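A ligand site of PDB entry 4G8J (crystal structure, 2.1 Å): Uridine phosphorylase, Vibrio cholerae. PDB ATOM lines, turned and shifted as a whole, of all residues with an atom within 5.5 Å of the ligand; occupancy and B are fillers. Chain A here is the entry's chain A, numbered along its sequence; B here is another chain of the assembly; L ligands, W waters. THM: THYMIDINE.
NE2 of Gln 165 lies within hydrogen-bond range of O2 of the ligand (2.7 Å).
A ring nitrogen (NE2) of His 7 of chain B is in hydrogen-bond range of an oxygen (O5') of the ligand, 2.8 Å away.
OE2 of Glu 197 lies within hydrogen-bond range of O3' of the ligand (2.8 Å).
An oxygen (O4') of the ligand lies within hydrogen-bond range of the side-chain hydroxyl (OG1) of Thr 93 (3.2 Å).
O4 of the ligand lies within hydrogen-bond range of NH2 of Arg 167 (2.8 Å).
NH2 of Arg 222 sits at hydrogen-bond distance from O of Gln 165 (2.8 Å).
O of Glu 226 is in hydrogen-bond range of NH2 of Arg 167 (2.7 Å).
The backbone NH (N) of Phe 161 lies close to the side-chain sulfur (SD) of Met 196 (3.7 Å).
The backbone carbonyl oxygen (O) of Phe 161 sits at hydrogen-bond distance from the guanidinium group (NH1) of Arg 167 (2.8 Å).
OE2 of Glu 197 is in hydrogen-bond range of N of Gly 69 (2.7 Å).
O of Gly 95 sits at hydrogen-bond distance from N of Phe 194, at 2.7 Å.
The side-chain carboxylate (OE2) of Glu 195 sits at hydrogen-bond distance from the backbone NH (N) of Glu 197.
The backbone carbonyl oxygen of Phe 194 lies within hydrogen-bond range of the side-chain hydroxyl of Thr 94, 2.5 Å away.
Residues that only touch the ligand: Thr 94 (3.9 Å), Gly 95 (3.6 Å), Phe 161 (3.5 Å), Phe 194 (3.7 Å), Glu 195 (3.1 Å), Met 196 (3.3 Å), Ile 219 (3.5 Å), Ile 220 (3.6 Å) and Arg 47 of chain B (3.2 Å).
Of the 23 residues printed, 14 come within 4 Å of the ligand.
Water W1 lies within hydrogen-bond range of OE1 of Gln 165, O4 of the ligand, NH2 of Arg 222 and NH1 of Arg 167.
Water W2 lies within hydrogen-bond range of the guanidinium group (NH2) of Arg 90 (2.7 Å), an oxygen (O3') of the ligand (2.8 Å), the side-chain carboxylate (OE2) of Glu 197 (3.1 Å) and the backbone carbonyl oxygen (O) of Gly 67 (3.2 Å).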
ATOM      1  N   GLY A  67       7.079  39.160 -18.673  1.00  0.00           N
ATOM      2  CA  GLY A  67       6.033  38.247 -18.253  1.00  0.00           C
ATOM      3  C   GLY A  67       5.549  37.482 -19.466  1.00  0.00           C
ATOM      4  O   GLY A  67       6.060  37.680 -20.577  1.00  0.00           O
ATOM      5  N   ILE A  68       4.575  36.601 -19.276  1.00  0.00           N
ATOM      6  CA  ILE A  68       4.037  35.830 -20.386  1.00  0.00           C
ATOM      7  C   ILE A  68       2.943  36.598 -21.122  1.00  0.00           C
ATOM      8  O   ILE A  68       2.040  37.154 -20.499  1.00  0.00           O
ATOM      9  CB  ILE A  68       3.448  34.478 -19.906  1.00  0.00           C
ATOM     10  CG1 ILE A  68       4.553  33.590 -19.337  1.00  0.00           C
ATOM     11  CG2 ILE A  68       2.733  33.771 -21.046  1.00  0.00           C
ATOM     12  CD1 ILE A  68       4.046  32.272 -18.783  1.00  0.00           C
ATOM     13  N   GLY A  69       3.045  36.632 -22.441  1.00  0.00           N
ATOM     14  CA  GLY A  69       1.968  37.134 -23.271  1.00  0.00           C
ATOM     15  C   GLY A  69       2.147  38.553 -23.773  1.00  0.00           C
ATOM     16  O   GLY A  69       2.870  39.352 -23.183  1.00  0.00           O
ATOM     17  N   ARG A  90      14.099  40.237 -28.100  1.00  0.00           N
ATOM     18  CA  ARG A  90      13.330  39.207 -27.436  1.00  0.00           C
ATOM     19  C   ARG A  90      14.090  37.885 -27.434  1.00  0.00           C
ATOM     20  O   ARG A  90      14.597  37.447 -28.460  1.00  0.00           O
ATOM     21  CB  ARG A  90      11.990  39.013 -28.139  1.00  0.00           C
ATOM     22  CG  ARG A  90      11.155  37.861 -27.602  1.00  0.00           C
ATOM     23  CD  ARG A  90      10.644  38.167 -26.200  1.00  0.00           C
ATOM     24  NE  ARG A  90       9.879  37.053 -25.651  1.00  0.00           N
ATOM     25  CZ  ARG A  90       9.337  37.050 -24.432  1.00  0.00           C
ATOM     26  NH1 ARG A  90       9.472  38.105 -23.647  1.00  0.00           N
ATOM     27  NH2 ARG A  90       8.671  35.992 -24.008  1.00  0.00           N
ATOM     28  N   THR A  93      11.906  30.701 -24.671  1.00  0.00           N
ATOM     29  CA  THR A  93      11.842  29.302 -25.072  1.00  0.00           C
ATOM     30  C   THR A  93      10.668  29.121 -26.024  1.00  0.00           C
ATOM     31  O   THR A  93       9.748  29.945 -26.046  1.00  0.00           O
ATOM     32  CB  THR A  93      11.666  28.373 -23.864  1.00  0.00           C
ATOM     33  OG1 THR A  93      10.474  28.718 -23.152  1.00  0.00           O
ATOM     34  CG2 THR A  93      12.863  28.485 -22.933  1.00  0.00           C
ATOM     35  N   THR A  94      10.694  28.054 -26.809  1.00  0.00           N
ATOM     36  CA  THR A  94       9.655  27.833 -27.795  1.00  0.00           C
ATOM     37  C   THR A  94       9.419  26.349 -28.062  1.00  0.00           C
ATOM     38  O   THR A  94      10.269  25.509 -27.758  1.00  0.00           O
ATOM     39  CB  THR A  94       9.994  28.537 -29.124  1.00  0.00           C
ATOM     40  OG1 THR A  94       8.863  28.491 -30.002  1.00  0.00           O
ATOM     41  CG2 THR A  94      11.184  27.859 -29.795  1.00  0.00           C
ATOM     42  N   GLY A  95       8.256  26.044 -28.606  1.00  0.00           N
ATOM     43  CA  GLY A  95       7.946  24.691 -29.048  1.00  0.00           C
ATOM     44  C   GLY A  95       7.942  24.638 -30.558  1.00  0.00           C
ATOM     45  O   GLY A  95       7.187  25.365 -31.199  1.00  0.00           O
ATOM     46  N   PHE A 161      -1.276  29.353 -24.178  1.00  0.00           N
ATOM     47  CA  PHE A 161      -0.282  28.281 -24.221  1.00  0.00           C
ATOM     48  C   PHE A 161      -0.950  26.980 -24.619  1.00  0.00           C
ATOM     49  O   PHE A 161      -0.319  26.105 -25.217  1.00  0.00           O
ATOM     50  CB  PHE A 161       0.383  28.134 -22.842  1.00  0.00           C
ATOM     51  CG  PHE A 161       1.467  27.096 -22.799  1.00  0.00           C
ATOM     52  CD1 PHE A 161       2.774  27.421 -23.155  1.00  0.00           C
ATOM     53  CD2 PHE A 161       1.191  25.803 -22.384  1.00  0.00           C
ATOM     54  CE1 PHE A 161       3.778  26.464 -23.109  1.00  0.00           C
ATOM     55  CE2 PHE A 161       2.195  24.836 -22.339  1.00  0.00           C
ATOM     56  CZ  PHE A 161       3.484  25.172 -22.706  1.00  0.00           C
ATOM     57  N   GLN A 165      -2.261  26.764 -29.112  1.00  0.00           N
ATOM     58  CA  GLN A 165      -1.156  25.959 -29.630  1.00  0.00           C
ATOM     59  C   GLN A 165      -1.635  24.523 -29.807  1.00  0.00           C
ATOM     60  O   GLN A 165      -0.844  23.587 -29.901  1.00  0.00           O
ATOM     61  CB  GLN A 165       0.051  26.071 -28.707  1.00  0.00           C
ATOM     62  CG  GLN A 165       0.459  27.514 -28.448  1.00  0.00           C
ATOM     63  CD  GLN A 165       1.734  27.652 -27.646  1.00  0.00           C
ATOM     64  OE1 GLN A 165       2.556  26.737 -27.592  1.00  0.00           O
ATOM     65  NE2 GLN A 165       1.915  28.817 -27.029  1.00  0.00           N
ATOM     66  N   ARG A 167      -3.096  22.253 -27.832  1.00  0.00           N
ATOM     67  CA  ARG A 167      -2.818  21.222 -26.850  1.00  0.00           C
ATOM     68  C   ARG A 167      -4.128  20.610 -26.379  1.00  0.00           C
ATOM     69  O   ARG A 167      -5.107  21.319 -26.132  1.00  0.00           O
ATOM     70  CB  ARG A 167      -2.041  21.795 -25.668  1.00  0.00           C
ATOM     71  CG  ARG A 167      -0.597  22.146 -25.983  1.00  0.00           C
ATOM     72  CD  ARG A 167       0.134  22.678 -24.769  1.00  0.00           C
ATOM     73  NE  ARG A 167       1.582  22.507 -24.890  1.00  0.00           N
ATOM     74  CZ  ARG A 167       2.408  23.418 -25.402  1.00  0.00           C
ATOM     75  NH1 ARG A 167       1.928  24.581 -25.849  1.00  0.00           N
ATOM     76  NH2 ARG A 167       3.706  23.165 -25.478  1.00  0.00           N
ATOM     77  N   PHE A 194       5.894  27.648 -31.950  1.00  0.00           N
ATOM     78  CA  PHE A 194       4.910  28.376 -31.157  1.00  0.00           C
ATOM     79  C   PHE A 194       5.612  29.165 -30.054  1.00  0.00           C
ATOM     80  O   PHE A 194       6.485  28.644 -29.365  1.00  0.00           O
ATOM     81  CB  PHE A 194       3.948  27.397 -30.476  1.00  0.00           C
ATOM     82  CG  PHE A 194       2.795  26.960 -31.328  1.00  0.00           C
ATOM     83  CD1 PHE A 194       1.880  27.880 -31.809  1.00  0.00           C
ATOM     84  CD2 PHE A 194       2.594  25.616 -31.604  1.00  0.00           C
ATOM     85  CE1 PHE A 194       0.809  27.468 -32.588  1.00  0.00           C
ATOM     86  CE2 PHE A 194       1.520  25.203 -32.373  1.00  0.00           C
ATOM     87  CZ  PHE A 194       0.627  26.123 -32.861  1.00  0.00           C
ATOM     88  N   GLU A 195       5.221  30.423 -29.887  1.00  0.00           N
ATOM     89  CA  GLU A 195       5.457  31.139 -28.641  1.00  0.00           C
ATOM     90  C   GLU A 195       4.315  32.123 -28.421  1.00  0.00           C
ATOM     91  O   GLU A 195       3.283  32.013 -29.077  1.00  0.00           O
ATOM     92  CB  GLU A 195       6.863  31.769 -28.571  1.00  0.00           C
ATOM     93  CG  GLU A 195       7.234  32.653 -29.734  1.00  0.00           C
ATOM     94  CD  GLU A 195       6.512  33.973 -29.720  1.00  0.00           C
ATOM     95  OE1 GLU A 195       5.588  34.152 -30.537  1.00  0.00           O
ATOM     96  OE2 GLU A 195       6.847  34.842 -28.877  1.00  0.00           O
ATOM     97  N   MET A 196       4.469  33.069 -27.497  1.00  0.00           N
ATOM     98  CA  MET A 196       3.307  33.851 -27.080  1.00  0.00           C
ATOM     99  C   MET A 196       3.484  35.369 -27.041  1.00  0.00           C
ATOM    100  O   MET A 196       2.612  36.073 -26.547  1.00  0.00           O
ATOM    101  CB  MET A 196       2.824  33.367 -25.708  1.00  0.00           C
ATOM    102  CG  MET A 196       2.388  31.909 -25.688  1.00  0.00           C
ATOM    103  SD  MET A 196       1.830  31.392 -24.066  1.00  0.00           S
ATOM    104  CE  MET A 196       0.462  32.515 -23.790  1.00  0.00           C
ATOM    105  N   GLU A 197       4.597  35.876 -27.565  1.00  0.00           N
ATOM    106  CA  GLU A 197       4.869  37.298 -27.428  1.00  0.00           C
ATOM    107  C   GLU A 197       5.295  37.998 -28.725  1.00  0.00           C
ATOM    108  O   GLU A 197       5.145  39.209 -28.850  1.00  0.00           O
ATOM    109  CB  GLU A 197       5.915  37.552 -26.337  1.00  0.00           C
ATOM    110  CG  GLU A 197       5.479  37.176 -24.923  1.00  0.00           C
ATOM    111  CD  GLU A 197       5.564  35.677 -24.661  1.00  0.00           C
ATOM    112  OE1 GLU A 197       6.232  34.972 -25.436  1.00  0.00           O
ATOM    113  OE2 GLU A 197       4.953  35.207 -23.670  1.00  0.00           O
ATOM    114  N   ILE A 219      12.855  23.981 -26.826  1.00  0.00           N
ATOM    115  CA  ILE A 219      12.962  23.073 -25.689  1.00  0.00           C
ATOM    116  C   ILE A 219      12.007  21.900 -25.817  1.00  0.00           C
ATOM    117  O   ILE A 219      12.049  20.962 -25.024  1.00  0.00           O
ATOM    118  CB  ILE A 219      12.682  23.801 -24.362  1.00  0.00           C
ATOM    119  CG1 ILE A 219      11.241  24.287 -24.314  1.00  0.00           C
ATOM    120  CG2 ILE A 219      13.662  24.961 -24.191  1.00  0.00           C
ATOM    121  CD1 ILE A 219      10.835  24.866 -22.973  1.00  0.00           C
ATOM    122  N   ILE A 220      11.149  21.949 -26.833  1.00  0.00           N
ATOM    123  CA  ILE A 220      10.235  20.854 -27.103  1.00  0.00           C
ATOM    124  C   ILE A 220       9.863  20.844 -28.581  1.00  0.00           C
ATOM    125  O   ILE A 220       9.729  21.893 -29.209  1.00  0.00           O
ATOM    126  CB  ILE A 220       8.973  20.929 -26.223  1.00  0.00           C
ATOM    127  CG1 ILE A 220       8.079  19.710 -26.436  1.00  0.00           C
ATOM    128  CG2 ILE A 220       8.197  22.216 -26.482  1.00  0.00           C
ATOM    129  CD1 ILE A 220       6.758  19.775 -25.707  1.00  0.00           C
ATOM    130  N   ARG A 222       6.799  19.703 -30.903  1.00  0.00           N
ATOM    131  CA  ARG A 222       5.388  19.342 -30.756  1.00  0.00           C
ATOM    132  C   ARG A 222       4.962  18.132 -31.580  1.00  0.00           C
ATOM    133  O   ARG A 222       3.855  17.614 -31.389  1.00  0.00           O
ATOM    134  CB  ARG A 222       4.506  20.552 -31.064  1.00  0.00           C
ATOM    135  CG  ARG A 222       4.607  21.653 -30.027  1.00  0.00           C
ATOM    136  CD  ARG A 222       4.010  21.194 -28.700  1.00  0.00           C
ATOM    137  NE  ARG A 222       2.664  20.681 -28.897  1.00  0.00           N
ATOM    138  CZ  ARG A 222       1.586  21.443 -29.024  1.00  0.00           C
ATOM    139  NH1 ARG A 222       0.389  20.887 -29.212  1.00  0.00           N
ATOM    140  NH2 ARG A 222       1.697  22.761 -28.976  1.00  0.00           N
ATOM    141  N   GLU A 226       3.342  17.098 -26.151  1.00  0.00           N
ATOM    142  CA  GLU A 226       2.693  18.382 -25.866  1.00  0.00           C
ATOM    143  C   GLU A 226       3.432  19.277 -24.874  1.00  0.00           C
ATOM    144  O   GLU A 226       3.559  20.481 -25.102  1.00  0.00           O
ATOM    145  CB  GLU A 226       1.250  18.172 -25.391  1.00  0.00           C
ATOM    146  CG  GLU A 226       0.276  17.858 -26.505  1.00  0.00           C
ATOM    147  CD  GLU A 226      -1.159  18.072 -26.097  1.00  0.00           C
ATOM    148  OE1 GLU A 226      -1.383  18.479 -24.932  1.00  0.00           O
ATOM    149  OE2 GLU A 226      -2.059  17.851 -26.922  1.00  0.00           O
ATOM    150  N   PRO A 228       6.880  19.913 -22.041  1.00  0.00           N
ATOM    151  CA  PRO A 228       8.228  19.541 -21.621  1.00  0.00           C
ATOM    152  C   PRO A 228       8.230  18.813 -20.287  1.00  0.00           C
ATOM    153  O   PRO A 228       7.479  19.202 -19.399  1.00  0.00           O
ATOM    154  CB  PRO A 228       8.942  20.887 -21.477  1.00  0.00           C
ATOM    155  CG  PRO A 228       8.147  21.836 -22.303  1.00  0.00           C
ATOM    156  CD  PRO A 228       6.726  21.375 -22.173  1.00  0.00           C
ATOM    157  N   PHE B   6       3.089  22.635 -15.623  1.00  0.00           N
ATOM    158  CA  PHE B   6       4.304  23.186 -16.221  1.00  0.00           C
ATOM    159  C   PHE B   6       4.681  24.586 -15.747  1.00  0.00           C
ATOM    160  O   PHE B   6       5.849  24.856 -15.468  1.00  0.00           O
ATOM    161  CB  PHE B   6       4.240  23.134 -17.740  1.00  0.00           C
ATOM    162  CG  PHE B   6       5.495  23.598 -18.419  1.00  0.00           C
ATOM    163  CD1 PHE B   6       6.678  22.912 -18.241  1.00  0.00           C
ATOM    164  CD2 PHE B   6       5.488  24.727 -19.226  1.00  0.00           C
ATOM    165  CE1 PHE B   6       7.842  23.334 -18.854  1.00  0.00           C
ATOM    166  CE2 PHE B   6       6.652  25.158 -19.839  1.00  0.00           C
ATOM    167  CZ  PHE B   6       7.834  24.462 -19.652  1.00  0.00           C
ATOM    168  N   HIS B   7       3.708  25.485 -15.660  1.00  0.00           N
ATOM    169  CA  HIS B   7       4.005  26.861 -15.269  1.00  0.00           C
ATOM    170  C   HIS B   7       3.892  27.106 -13.764  1.00  0.00           C
ATOM    171  O   HIS B   7       4.761  27.732 -13.163  1.00  0.00           O
ATOM    172  CB  HIS B   7       3.131  27.857 -16.033  1.00  0.00           C
ATOM    173  CG  HIS B   7       3.355  27.850 -17.509  1.00  0.00           C
ATOM    174  ND1 HIS B   7       2.725  26.954 -18.344  1.00  0.00           N
ATOM    175  CD2 HIS B   7       4.146  28.616 -18.296  1.00  0.00           C
ATOM    176  CE1 HIS B   7       3.115  27.171 -19.592  1.00  0.00           C
ATOM    177  NE2 HIS B   7       3.982  28.172 -19.587  1.00  0.00           N
ATOM    178  N   ARG B  47       7.897  32.519 -12.428  1.00  0.00           N
ATOM    179  CA  ARG B  47       7.502  33.635 -13.280  1.00  0.00           C
ATOM    180  C   ARG B  47       6.560  34.585 -12.529  1.00  0.00           C
ATOM    181  O   ARG B  47       6.822  34.937 -11.381  1.00  0.00           O
ATOM    182  CB  ARG B  47       6.842  33.116 -14.564  1.00  0.00           C
ATOM    183  CG  ARG B  47       7.761  32.253 -15.425  1.00  0.00           C
ATOM    184  CD  ARG B  47       7.013  31.659 -16.604  1.00  0.00           C
ATOM    185  NE  ARG B  47       7.895  30.960 -17.531  1.00  0.00           N
ATOM    186  CZ  ARG B  47       8.495  31.534 -18.578  1.00  0.00           C
ATOM    187  NH1 ARG B  47       8.304  32.823 -18.826  1.00  0.00           N
ATOM    188  NH2 ARG B  47       9.277  30.818 -19.369  1.00  0.00           N
ATOM    189  N   ILE B  75      -3.219  30.570 -18.637  1.00  0.00           N
ATOM    190  CA  ILE B  75      -2.320  29.513 -18.207  1.00  0.00           C
ATOM    191  C   ILE B  75      -2.609  29.123 -16.763  1.00  0.00           C
ATOM    192  O   ILE B  75      -2.767  27.944 -16.446  1.00  0.00           O
ATOM    193  CB  ILE B  75      -0.849  29.943 -18.342  1.00  0.00           C
ATOM    194  CG1 ILE B  75      -0.471  30.054 -19.820  1.00  0.00           C
ATOM    195  CG2 ILE B  75       0.062  28.969 -17.622  1.00  0.00           C
ATOM    196  CD1 ILE B  75       0.926  30.571 -20.062  1.00  0.00           C
HETATM  197  O5' THM L   1       5.860  28.980 -21.505  1.00  0.00           O
HETATM  198  C5' THM L   1       6.898  29.843 -21.221  1.00  0.00           C
HETATM  199  C4' THM L   1       7.157  30.728 -22.379  1.00  0.00           C
HETATM  200  O4' THM L   1       7.548  29.975 -23.489  1.00  0.00           O
HETATM  201  C3' THM L   1       5.929  31.484 -22.731  1.00  0.00           C
HETATM  202  O3' THM L   1       6.255  32.804 -22.925  1.00  0.00           O
HETATM  203  C2' THM L   1       5.431  30.871 -23.967  1.00  0.00           C
HETATM  204  C1' THM L   1       6.610  30.105 -24.503  1.00  0.00           C
HETATM  205  N1  THM L   1       6.310  28.776 -25.013  1.00  0.00           N
HETATM  206  C2  THM L   1       5.193  28.519 -25.881  1.00  0.00           C
HETATM  207  O2  THM L   1       4.440  29.420 -26.219  1.00  0.00           O
HETATM  208  N3  THM L   1       4.949  27.207 -26.353  1.00  0.00           N
HETATM  209  C4  THM L   1       5.784  26.153 -25.971  1.00  0.00           C
HETATM  210  O4  THM L   1       5.564  25.017 -26.379  1.00  0.00           O
HETATM  211  C5  THM L   1       6.939  26.409 -25.088  1.00  0.00           C
HETATM  212  C5M THM L   1       7.831  25.313 -24.691  1.00  0.00           C
HETATM  213  C6  THM L   1       7.174  27.692 -24.630  1.00  0.00           C
HETATM  214  O   HOH W   1       3.812  24.597 -28.447  1.00  0.00           O
HETATM  215  O   HOH W   2       7.394  35.087 -21.769  1.00  0.00           O
HETATM  216  O   HOH W   3       9.300  27.328 -21.219  1.00  0.00           O
